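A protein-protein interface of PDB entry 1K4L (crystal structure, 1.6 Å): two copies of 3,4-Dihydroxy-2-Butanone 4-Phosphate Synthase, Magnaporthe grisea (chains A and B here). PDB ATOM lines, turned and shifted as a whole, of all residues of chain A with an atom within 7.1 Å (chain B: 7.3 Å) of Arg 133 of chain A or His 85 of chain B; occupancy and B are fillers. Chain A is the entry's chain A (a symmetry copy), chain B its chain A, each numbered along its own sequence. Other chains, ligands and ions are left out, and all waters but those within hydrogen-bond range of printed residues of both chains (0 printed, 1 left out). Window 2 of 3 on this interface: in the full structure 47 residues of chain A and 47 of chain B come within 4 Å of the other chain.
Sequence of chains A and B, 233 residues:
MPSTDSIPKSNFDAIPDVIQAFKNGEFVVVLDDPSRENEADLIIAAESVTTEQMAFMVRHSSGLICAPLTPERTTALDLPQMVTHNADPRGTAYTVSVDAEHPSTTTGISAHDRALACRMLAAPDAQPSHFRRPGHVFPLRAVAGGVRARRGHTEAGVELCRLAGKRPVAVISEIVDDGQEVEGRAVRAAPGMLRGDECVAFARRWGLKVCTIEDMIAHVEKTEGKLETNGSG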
ATOM      1  N   LEU A  77     -38.228  -8.092  -7.271  1.00  0.00           N
ATOM      2  CA  LEU A  77     -37.504  -7.342  -8.265  1.00  0.00           C
ATOM      3  C   LEU A  77     -36.025  -7.621  -8.305  1.00  0.00           C
ATOM      4  O   LEU A  77     -35.298  -6.973  -9.092  1.00  0.00           O
ATOM      5  CB  LEU A  77     -37.785  -5.820  -8.143  1.00  0.00           C
ATOM      6  CG  LEU A  77     -39.265  -5.392  -8.245  1.00  0.00           C
ATOM      7  CD1 LEU A  77     -39.388  -3.877  -7.993  1.00  0.00           C
ATOM      8  CD2 LEU A  77     -39.848  -5.826  -9.603  1.00  0.00           C
ATOM      9  N   ASP A  78     -35.631  -8.600  -7.476  1.00  0.00           N
ATOM     10  CA  ASP A  78     -34.242  -9.036  -7.446  1.00  0.00           C
ATOM     11  C   ASP A  78     -33.280  -7.870  -7.156  1.00  0.00           C
ATOM     12  O   ASP A  78     -32.412  -7.493  -7.962  1.00  0.00           O
ATOM     13  CB  ASP A  78     -33.887  -9.610  -8.827  1.00  0.00           C
ATOM     14  CG  ASP A  78     -32.681 -10.480  -8.651  1.00  0.00           C
ATOM     15  OD1 ASP A  78     -32.139 -10.638  -7.581  1.00  0.00           O
ATOM     16  OD2 ASP A  78     -32.347 -11.113  -9.728  1.00  0.00           O
ATOM     17  N   LEU A  79     -33.469  -7.346  -5.969  1.00  0.00           N
ATOM     18  CA  LEU A  79     -32.641  -6.247  -5.502  1.00  0.00           C
ATOM     19  C   LEU A  79     -31.904  -6.687  -4.266  1.00  0.00           C
ATOM     20  O   LEU A  79     -32.339  -6.495  -3.132  1.00  0.00           O
ATOM     21  CB  LEU A  79     -33.497  -4.986  -5.183  1.00  0.00           C
ATOM     22  CG  LEU A  79     -34.250  -4.478  -6.420  1.00  0.00           C
ATOM     23  CD1 LEU A  79     -35.279  -3.433  -5.998  1.00  0.00           C
ATOM     24  CD2 LEU A  79     -33.357  -3.940  -7.536  1.00  0.00           C
ATOM     25  N   PRO A  80     -30.732  -7.281  -4.471  1.00  0.00           N
ATOM     26  CA  PRO A  80     -29.939  -7.740  -3.330  1.00  0.00           C
ATOM     27  C   PRO A  80     -29.403  -6.568  -2.475  1.00  0.00           C
ATOM     28  O   PRO A  80     -29.229  -5.463  -3.001  1.00  0.00           O
ATOM     29  CB  PRO A  80     -28.750  -8.465  -3.993  1.00  0.00           C
ATOM     30  CG  PRO A  80     -28.744  -8.129  -5.476  1.00  0.00           C
ATOM     31  CD  PRO A  80     -30.129  -7.531  -5.793  1.00  0.00           C
ATOM     32  N   VAL A  96     -28.691  -2.804  -3.981  1.00  0.00           N
ATOM     33  CA  VAL A  96     -27.782  -2.399  -5.012  1.00  0.00           C
ATOM     34  C   VAL A  96     -28.560  -1.245  -5.670  1.00  0.00           C
ATOM     35  O   VAL A  96     -29.802  -1.219  -5.638  1.00  0.00           O
ATOM     36  CB  VAL A  96     -27.543  -3.595  -5.935  1.00  0.00           C
ATOM     37  CG1 VAL A  96     -28.857  -4.081  -6.525  1.00  0.00           C
ATOM     38  CG2 VAL A  96     -26.641  -3.246  -7.096  1.00  0.00           C
ATOM     39  N   SER A  97     -27.847  -0.269  -6.236  1.00  0.00           N
ATOM     40  CA  SER A  97     -28.493   0.899  -6.861  1.00  0.00           C
ATOM     41  C   SER A  97     -29.046   0.576  -8.231  1.00  0.00           C
ATOM     42  O   SER A  97     -28.615  -0.390  -8.842  1.00  0.00           O
ATOM     43  CB  SER A  97     -27.547   2.116  -6.879  1.00  0.00           C
ATOM     44  OG  SER A  97     -26.453   1.821  -7.733  1.00  0.00           O
ATOM     45  N   VAL A  98     -29.951   1.431  -8.761  1.00  0.00           N
ATOM     46  CA  VAL A  98     -30.489   1.149 -10.073  1.00  0.00           C
ATOM     47  C   VAL A  98     -30.822   2.399 -10.873  1.00  0.00           C
ATOM     48  O   VAL A  98     -31.044   3.519 -10.318  1.00  0.00           O
ATOM     49  CB  VAL A  98     -31.866   0.423  -9.915  1.00  0.00           C
ATOM     50  CG1 VAL A  98     -31.786  -0.915  -9.165  1.00  0.00           C
ATOM     51  CG2 VAL A  98     -32.862   1.374  -9.204  1.00  0.00           C
ATOM     52  N   ASP A  99     -30.926   2.107 -12.171  1.00  0.00           N
ATOM     53  CA  ASP A  99     -31.403   3.000 -13.197  1.00  0.00           C
ATOM     54  C   ASP A  99     -32.596   2.294 -13.879  1.00  0.00           C
ATOM     55  O   ASP A  99     -32.755   1.062 -13.803  1.00  0.00           O
ATOM     56  CB  ASP A  99     -30.366   3.292 -14.270  1.00  0.00           C
ATOM     57  CG  ASP A  99     -29.462   4.426 -13.801  1.00  0.00           C
ATOM     58  OD1 ASP A  99     -29.536   4.919 -12.700  1.00  0.00           O
ATOM     59  OD2 ASP A  99     -28.576   4.733 -14.677  1.00  0.00           O
ATOM     60  N   GLN A 127     -40.594  -5.810 -13.223  1.00  0.00           N
ATOM     61  CA  GLN A 127     -39.791  -7.016 -13.282  1.00  0.00           C
ATOM     62  C   GLN A 127     -38.309  -6.677 -13.074  1.00  0.00           C
ATOM     63  O   GLN A 127     -37.868  -5.589 -13.439  1.00  0.00           O
ATOM     64  CB  GLN A 127     -39.830  -7.608 -14.717  1.00  0.00           C
ATOM     65  CG  GLN A 127     -41.230  -8.032 -15.156  1.00  0.00           C
ATOM     66  CD  GLN A 127     -41.679  -9.204 -14.308  1.00  0.00           C
ATOM     67  OE1 GLN A 127     -41.359  -9.306 -13.112  1.00  0.00           O
ATOM     68  NE2 GLN A 127     -42.343 -10.162 -14.968  1.00  0.00           N
ATOM     69  N   PRO A 128     -37.520  -7.648 -12.612  1.00  0.00           N
ATOM     70  CA  PRO A 128     -36.089  -7.408 -12.415  1.00  0.00           C
ATOM     71  C   PRO A 128     -35.359  -6.768 -13.594  1.00  0.00           C
ATOM     72  O   PRO A 128     -34.500  -5.899 -13.406  1.00  0.00           O
ATOM     73  CB  PRO A 128     -35.500  -8.798 -12.091  1.00  0.00           C
ATOM     74  CG  PRO A 128     -36.639  -9.522 -11.400  1.00  0.00           C
ATOM     75  CD  PRO A 128     -37.874  -9.024 -12.143  1.00  0.00           C
ATOM     76  N   SER A 129     -35.689  -7.193 -14.811  1.00  0.00           N
ATOM     77  CA  SER A 129     -35.083  -6.718 -16.067  1.00  0.00           C
ATOM     78  C   SER A 129     -35.432  -5.257 -16.399  1.00  0.00           C
ATOM     79  O   SER A 129     -34.853  -4.684 -17.356  1.00  0.00           O
ATOM     80  CB  SER A 129     -35.425  -7.587 -17.295  1.00  0.00           C
ATOM     81  OG  SER A 129     -36.841  -7.669 -17.422  1.00  0.00           O
ATOM     82  N   HIS A 130     -36.364  -4.696 -15.617  1.00  0.00           N
ATOM     83  CA  HIS A 130     -36.733  -3.306 -15.819  1.00  0.00           C
ATOM     84  C   HIS A 130     -35.662  -2.334 -15.278  1.00  0.00           C
ATOM     85  O   HIS A 130     -35.682  -1.115 -15.558  1.00  0.00           O
ATOM     86  CB  HIS A 130     -38.013  -3.015 -15.032  1.00  0.00           C
ATOM     87  CG  HIS A 130     -39.165  -3.582 -15.771  1.00  0.00           C
ATOM     88  ND1 HIS A 130     -40.425  -3.641 -15.201  1.00  0.00           N
ATOM     89  CD2 HIS A 130     -39.218  -4.134 -17.019  1.00  0.00           C
ATOM     90  CE1 HIS A 130     -41.219  -4.199 -16.109  1.00  0.00           C
ATOM     91  NE2 HIS A 130     -40.538  -4.531 -17.208  1.00  0.00           N
ATOM     92  N   PHE A 131     -34.758  -2.860 -14.442  1.00  0.00           N
ATOM     93  CA  PHE A 131     -33.755  -1.973 -13.837  1.00  0.00           C
ATOM     94  C   PHE A 131     -32.301  -2.367 -14.185  1.00  0.00           C
ATOM     95  O   PHE A 131     -31.975  -3.575 -14.279  1.00  0.00           O
ATOM     96  CB  PHE A 131     -33.926  -2.073 -12.319  1.00  0.00           C
ATOM     97  CG  PHE A 131     -35.384  -1.921 -11.982  1.00  0.00           C
ATOM     98  CD1 PHE A 131     -36.237  -3.013 -11.784  1.00  0.00           C
ATOM     99  CD2 PHE A 131     -35.904  -0.625 -11.950  1.00  0.00           C
ATOM    100  CE1 PHE A 131     -37.599  -2.831 -11.493  1.00  0.00           C
ATOM    101  CE2 PHE A 131     -37.271  -0.420 -11.680  1.00  0.00           C
ATOM    102  CZ  PHE A 131     -38.092  -1.524 -11.493  1.00  0.00           C
ATOM    103  N   ARG A 132     -31.431  -1.349 -14.366  1.00  0.00           N
ATOM    104  CA  ARG A 132     -30.003  -1.563 -14.606  1.00  0.00           C
ATOM    105  C   ARG A 132     -29.319  -1.425 -13.253  1.00  0.00           C
ATOM    106  O   ARG A 132     -29.666  -0.548 -12.444  1.00  0.00           O
ATOM    107  CB  ARG A 132     -29.469  -0.477 -15.508  1.00  0.00           C
ATOM    108  CG  ARG A 132     -30.227  -0.329 -16.797  1.00  0.00           C
ATOM    109  CD  ARG A 132     -29.607   0.717 -17.705  1.00  0.00           C
ATOM    110  NE  ARG A 132     -30.335   0.786 -18.956  1.00  0.00           N
ATOM    111  CZ  ARG A 132     -30.316   1.826 -19.754  1.00  0.00           C
ATOM    112  NH1 ARG A 132     -29.580   2.877 -19.428  1.00  0.00           N
ATOM    113  NH2 ARG A 132     -31.043   1.812 -20.876  1.00  0.00           N
ATOM    114  N   ARG A 133     -28.384  -2.314 -12.933  1.00  0.00           N
ATOM    115  CA  ARG A 133     -27.673  -2.238 -11.692  1.00  0.00           C
ATOM    116  C   ARG A 133     -26.186  -2.190 -12.055  1.00  0.00           C
ATOM    117  O   ARG A 133     -25.718  -2.964 -12.895  1.00  0.00           O
ATOM    118  CB  ARG A 133     -27.924  -3.363 -10.694  1.00  0.00           C
ATOM    119  CG  ARG A 133     -29.388  -3.872 -10.594  1.00  0.00           C
ATOM    120  CD  ARG A 133     -29.771  -4.770 -11.819  1.00  0.00           C
ATOM    121  NE  ARG A 133     -31.204  -5.178 -11.907  1.00  0.00           N
ATOM    122  CZ  ARG A 133     -31.775  -5.768 -10.870  1.00  0.00           C
ATOM    123  NH1 ARG A 133     -31.033  -6.030  -9.763  1.00  0.00           N
ATOM    124  NH2 ARG A 133     -33.084  -6.079 -10.940  1.00  0.00           N
ATOM    125  N   PRO A 134     -25.395  -1.266 -11.474  1.00  0.00           N
ATOM    126  CA  PRO A 134     -25.799  -0.298 -10.471  1.00  0.00           C
ATOM    127  C   PRO A 134     -26.381   0.909 -11.209  1.00  0.00           C
ATOM    128  O   PRO A 134     -26.468   0.957 -12.451  1.00  0.00           O
ATOM    129  CB  PRO A 134     -24.477   0.101  -9.757  1.00  0.00           C
ATOM    130  CG  PRO A 134     -23.451  -0.005 -10.885  1.00  0.00           C
ATOM    131  CD  PRO A 134     -23.946  -1.096 -11.861  1.00  0.00           C
ATOM    132  N   GLY A 135     -26.803   1.891 -10.415  1.00  0.00           N
ATOM    133  CA  GLY A 135     -27.387   3.067 -11.023  1.00  0.00           C
ATOM    134  C   GLY A 135     -27.386   4.262 -10.073  1.00  0.00           C
ATOM    135  O   GLY A 135     -26.489   4.411  -9.229  1.00  0.00           O
ATOM    136  N   MET B  82     -19.420  -2.390  -6.173  1.00  0.00           N
ATOM    137  CA  MET B  82     -20.768  -2.569  -5.677  1.00  0.00           C
ATOM    138  C   MET B  82     -21.421  -3.808  -6.294  1.00  0.00           C
ATOM    139  O   MET B  82     -22.209  -4.528  -5.642  1.00  0.00           O
ATOM    140  CB  MET B  82     -21.623  -1.377  -6.147  1.00  0.00           C
ATOM    141  CG  MET B  82     -22.905  -1.328  -5.325  1.00  0.00           C
ATOM    142  SD  MET B  82     -23.955   0.035  -5.902  1.00  0.00           S
ATOM    143  CE  MET B  82     -23.129   1.490  -5.212  1.00  0.00           C
ATOM    144  N   VAL B  83     -21.134  -3.962  -7.558  1.00  0.00           N
ATOM    145  CA  VAL B  83     -21.682  -5.105  -8.228  1.00  0.00           C
ATOM    146  C   VAL B  83     -20.640  -5.907  -9.002  1.00  0.00           C
ATOM    147  O   VAL B  83     -19.687  -5.368  -9.588  1.00  0.00           O
ATOM    148  CB  VAL B  83     -22.867  -4.801  -9.133  1.00  0.00           C
ATOM    149  CG1 VAL B  83     -23.883  -3.823  -8.524  1.00  0.00           C
ATOM    150  CG2 VAL B  83     -22.399  -4.404 -10.510  1.00  0.00           C
ATOM    151  N   THR B  84     -20.871  -7.221  -9.042  1.00  0.00           N
ATOM    152  CA  THR B  84     -20.006  -8.069  -9.801  1.00  0.00           C
ATOM    153  C   THR B  84     -20.351  -8.016 -11.257  1.00  0.00           C
ATOM    154  O   THR B  84     -19.486  -8.035 -12.088  1.00  0.00           O
ATOM    155  CB  THR B  84     -20.084  -9.489  -9.292  1.00  0.00           C
ATOM    156  OG1 THR B  84     -21.443  -9.884  -9.435  1.00  0.00           O
ATOM    157  CG2 THR B  84     -19.613  -9.399  -7.838  1.00  0.00           C
ATOM    158  N   HIS B  85     -21.608  -7.953 -11.623  1.00  0.00           N
ATOM    159  CA  HIS B  85     -21.861  -7.903 -13.050  1.00  0.00           C
ATOM    160  C   HIS B  85     -22.481  -6.556 -13.360  1.00  0.00           C
ATOM    161  O   HIS B  85     -23.708  -6.393 -13.316  1.00  0.00           O
ATOM    162  CB  HIS B  85     -22.747  -9.061 -13.520  1.00  0.00           C
ATOM    163  CG  HIS B  85     -22.293 -10.436 -13.068  1.00  0.00           C
ATOM    164  ND1 HIS B  85     -21.740 -11.366 -13.961  1.00  0.00           N
ATOM    165  CD2 HIS B  85     -22.373 -11.055 -11.841  1.00  0.00           C
ATOM    166  CE1 HIS B  85     -21.463 -12.471 -13.268  1.00  0.00           C
ATOM    167  NE2 HIS B  85     -21.854 -12.327 -11.999  1.00  0.00           N
ATOM    168  N   ASN B  86     -21.588  -5.597 -13.610  1.00  0.00           N
ATOM    169  CA  ASN B  86     -21.926  -4.205 -13.873  1.00  0.00           C
ATOM    170  C   ASN B  86     -22.773  -3.984 -15.108  1.00  0.00           C
ATOM    171  O   ASN B  86     -22.282  -4.164 -16.223  1.00  0.00           O
ATOM    172  CB  ASN B  86     -20.691  -3.307 -13.865  1.00  0.00           C
ATOM    173  CG  ASN B  86     -21.073  -1.855 -13.681  1.00  0.00           C
ATOM    174  OD1 ASN B  86     -21.955  -1.344 -14.403  1.00  0.00           O
ATOM    175  ND2 ASN B  86     -20.407  -1.189 -12.723  1.00  0.00           N
ATOM    176  N   ALA B  87     -24.049  -3.598 -14.850  1.00  0.00           N
ATOM    177  CA  ALA B  87     -25.083  -3.341 -15.849  1.00  0.00           C
ATOM    178  C   ALA B  87     -25.132  -1.891 -16.361  1.00  0.00           C
ATOM    179  O   ALA B  87     -25.886  -1.601 -17.287  1.00  0.00           O
ATOM    180  CB  ALA B  87     -26.454  -3.941 -15.505  1.00  0.00           C
ATOM    181  N   ASP B  88     -24.335  -0.990 -15.776  1.00  0.00           N
ATOM    182  CA  ASP B  88     -24.219   0.400 -16.249  1.00  0.00           C
ATOM    183  C   ASP B  88     -23.605   0.418 -17.669  1.00  0.00           C
ATOM    184  O   ASP B  88     -22.591  -0.250 -17.965  1.00  0.00           O
ATOM    185  CB  ASP B  88     -23.386   1.248 -15.275  1.00  0.00           C
ATOM    186  CG  ASP B  88     -23.222   2.679 -15.718  1.00  0.00           C
ATOM    187  OD1 ASP B  88     -22.693   3.009 -16.766  1.00  0.00           O
ATOM    188  OD2 ASP B  88     -23.761   3.493 -14.841  1.00  0.00           O
ATOM    189  N   PRO B  89     -24.228   1.144 -18.600  1.00  0.00           N
ATOM    190  CA  PRO B  89     -23.745   1.135 -19.978  1.00  0.00           C
ATOM    191  C   PRO B  89     -22.371   1.742 -20.151  1.00  0.00           C
ATOM    192  O   PRO B  89     -21.689   1.486 -21.146  1.00  0.00           O
ATOM    193  CB  PRO B  89     -24.814   1.794 -20.848  1.00  0.00           C
ATOM    194  CG  PRO B  89     -25.986   2.134 -19.918  1.00  0.00           C
ATOM    195  CD  PRO B  89     -25.497   1.929 -18.477  1.00  0.00           C
ATOM    196  N   TYR B  94     -18.724   2.005  -9.626  1.00  0.00           N
ATOM    197  CA  TYR B  94     -18.996   2.189  -8.221  1.00  0.00           C
ATOM    198  C   TYR B  94     -18.448   1.154  -7.242  1.00  0.00           C
ATOM    199  O   TYR B  94     -18.689  -0.043  -7.400  1.00  0.00           O
ATOM    200  CB  TYR B  94     -20.526   2.123  -7.886  1.00  0.00           C
ATOM    201  CG  TYR B  94     -21.276   3.130  -8.658  1.00  0.00           C
ATOM    202  CD1 TYR B  94     -21.813   2.839  -9.906  1.00  0.00           C
ATOM    203  CD2 TYR B  94     -21.382   4.407  -8.102  1.00  0.00           C
ATOM    204  CE1 TYR B  94     -22.530   3.824 -10.597  1.00  0.00           C
ATOM    205  CE2 TYR B  94     -22.055   5.404  -8.811  1.00  0.00           C
ATOM    206  CZ  TYR B  94     -22.626   5.106 -10.040  1.00  0.00           C
ATOM    207  OH  TYR B  94     -23.248   6.165 -10.683  1.00  0.00           O
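Among the printed residues, merely in contact across the chains: Val 96 of chain A with Val 83 of chain B (3.2 Å), Pro 134 of chain A with Asn 86 of chain B (3.2 Å), Pro 134 of chain A with Tyr 94 of chain B (3.4 Å), Arg 132 of chain A with Pro 89 of chain B (3.7 Å), Arg 133 of chain A with Asp 88 of chain B (3.8 Å), Arg 133 of chain A with Asn 86 of chain B (3.8 Å), Pro 134 of chain A with Met 82 of chain B (3.9 Å), Pro 134 of chain A with Val 83 of chain B (3.9 Å), Pro 134 of chain A with Ala 87 of chain B (3.9 Å), Pro 134 of chain A with Asp 88 of chain B (3.9 Å), Gly 135 of chain A with Tyr 94 of chain B (3.96 Å) and Arg 133 of chain A with His 85 of chain B (3.997 Å).
Leu 79 of chain A touches none of the printed residues of chain B. Of the printed residues of chain B, Val 96 of chain A touches Val 83. Printed residues of chain B within 4 Å of Ser 97 of chain A: Met 82. Of the printed residues of chain B, Arg 133 of chain A touches His 85, Asn 86, Ala 87 and Asp 88. Of the printed residues of chain B, Pro 134 of chain A touches Met 82, Val 83, Asn 86, Ala 87, Asp 88 and Tyr 94. Of the printed residues of chain A, His 85 of chain B touches Arg 133. Of the printed residues of chain A, Asn 86 of chain B touches Arg 133 and Pro 134. Of the printed residues of chain A, Ala 87 of chain B touches Arg 133 and Pro 134.
No position is printed for both chains. Of the 14 pairs that touch across the chains among the printed residues, none has its exchanged pair printed and touching as well.
Of the 17 printed residues of chain A, 6 touch a printed residue of chain B. Printed residues of chain A that touch a printed residue of chain B: Val 96, Ser 97, Arg 132, Arg 133, Pro 134 and Gly 135. Along chain A the printed residues that touch a printed residue of chain B span positions 96 to 135. Among the printed residues, 14 pairs touch across the chains.
The backbone carbonyl oxygen (O) of Pro 128 of chain A sits at hydrogen-bond distance from the guanidinium group (NH2) of Arg 133 of chain A (2.8 Å). The side-chain hydroxyl (OG) of Ser 97 of chain A sits at hydrogen-bond distance from the backbone NH (N) of Gly 135 of chain A (2.7 Å). N of Arg 132 of chain A sits at hydrogen-bond distance from O of Asp 99 of chain A, at 2.8 Å. O of Phe 131 of chain A sits at hydrogen-bond distance from NE of Arg 133 of chain A (3.0 Å). The backbone carbonyl oxygen (O) of Leu 77 of chain A is in hydrogen-bond range of the guanidinium group (NH2) of Arg 133 of chain A (3.0 Å). O of Pro 80 of chain A is in hydrogen-bond range of N of Val 96 of chain A, at 2.9 Å.
O of Arg 133 of chain A lies within hydrogen-bond range of N of Ala 87 of chain B. The side-chain hydroxyl (OG) of Ser 97 of chain A is in hydrogen-bond range of the side-chain sulfur (SD) of Met 82 of chain B (3.6 Å).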
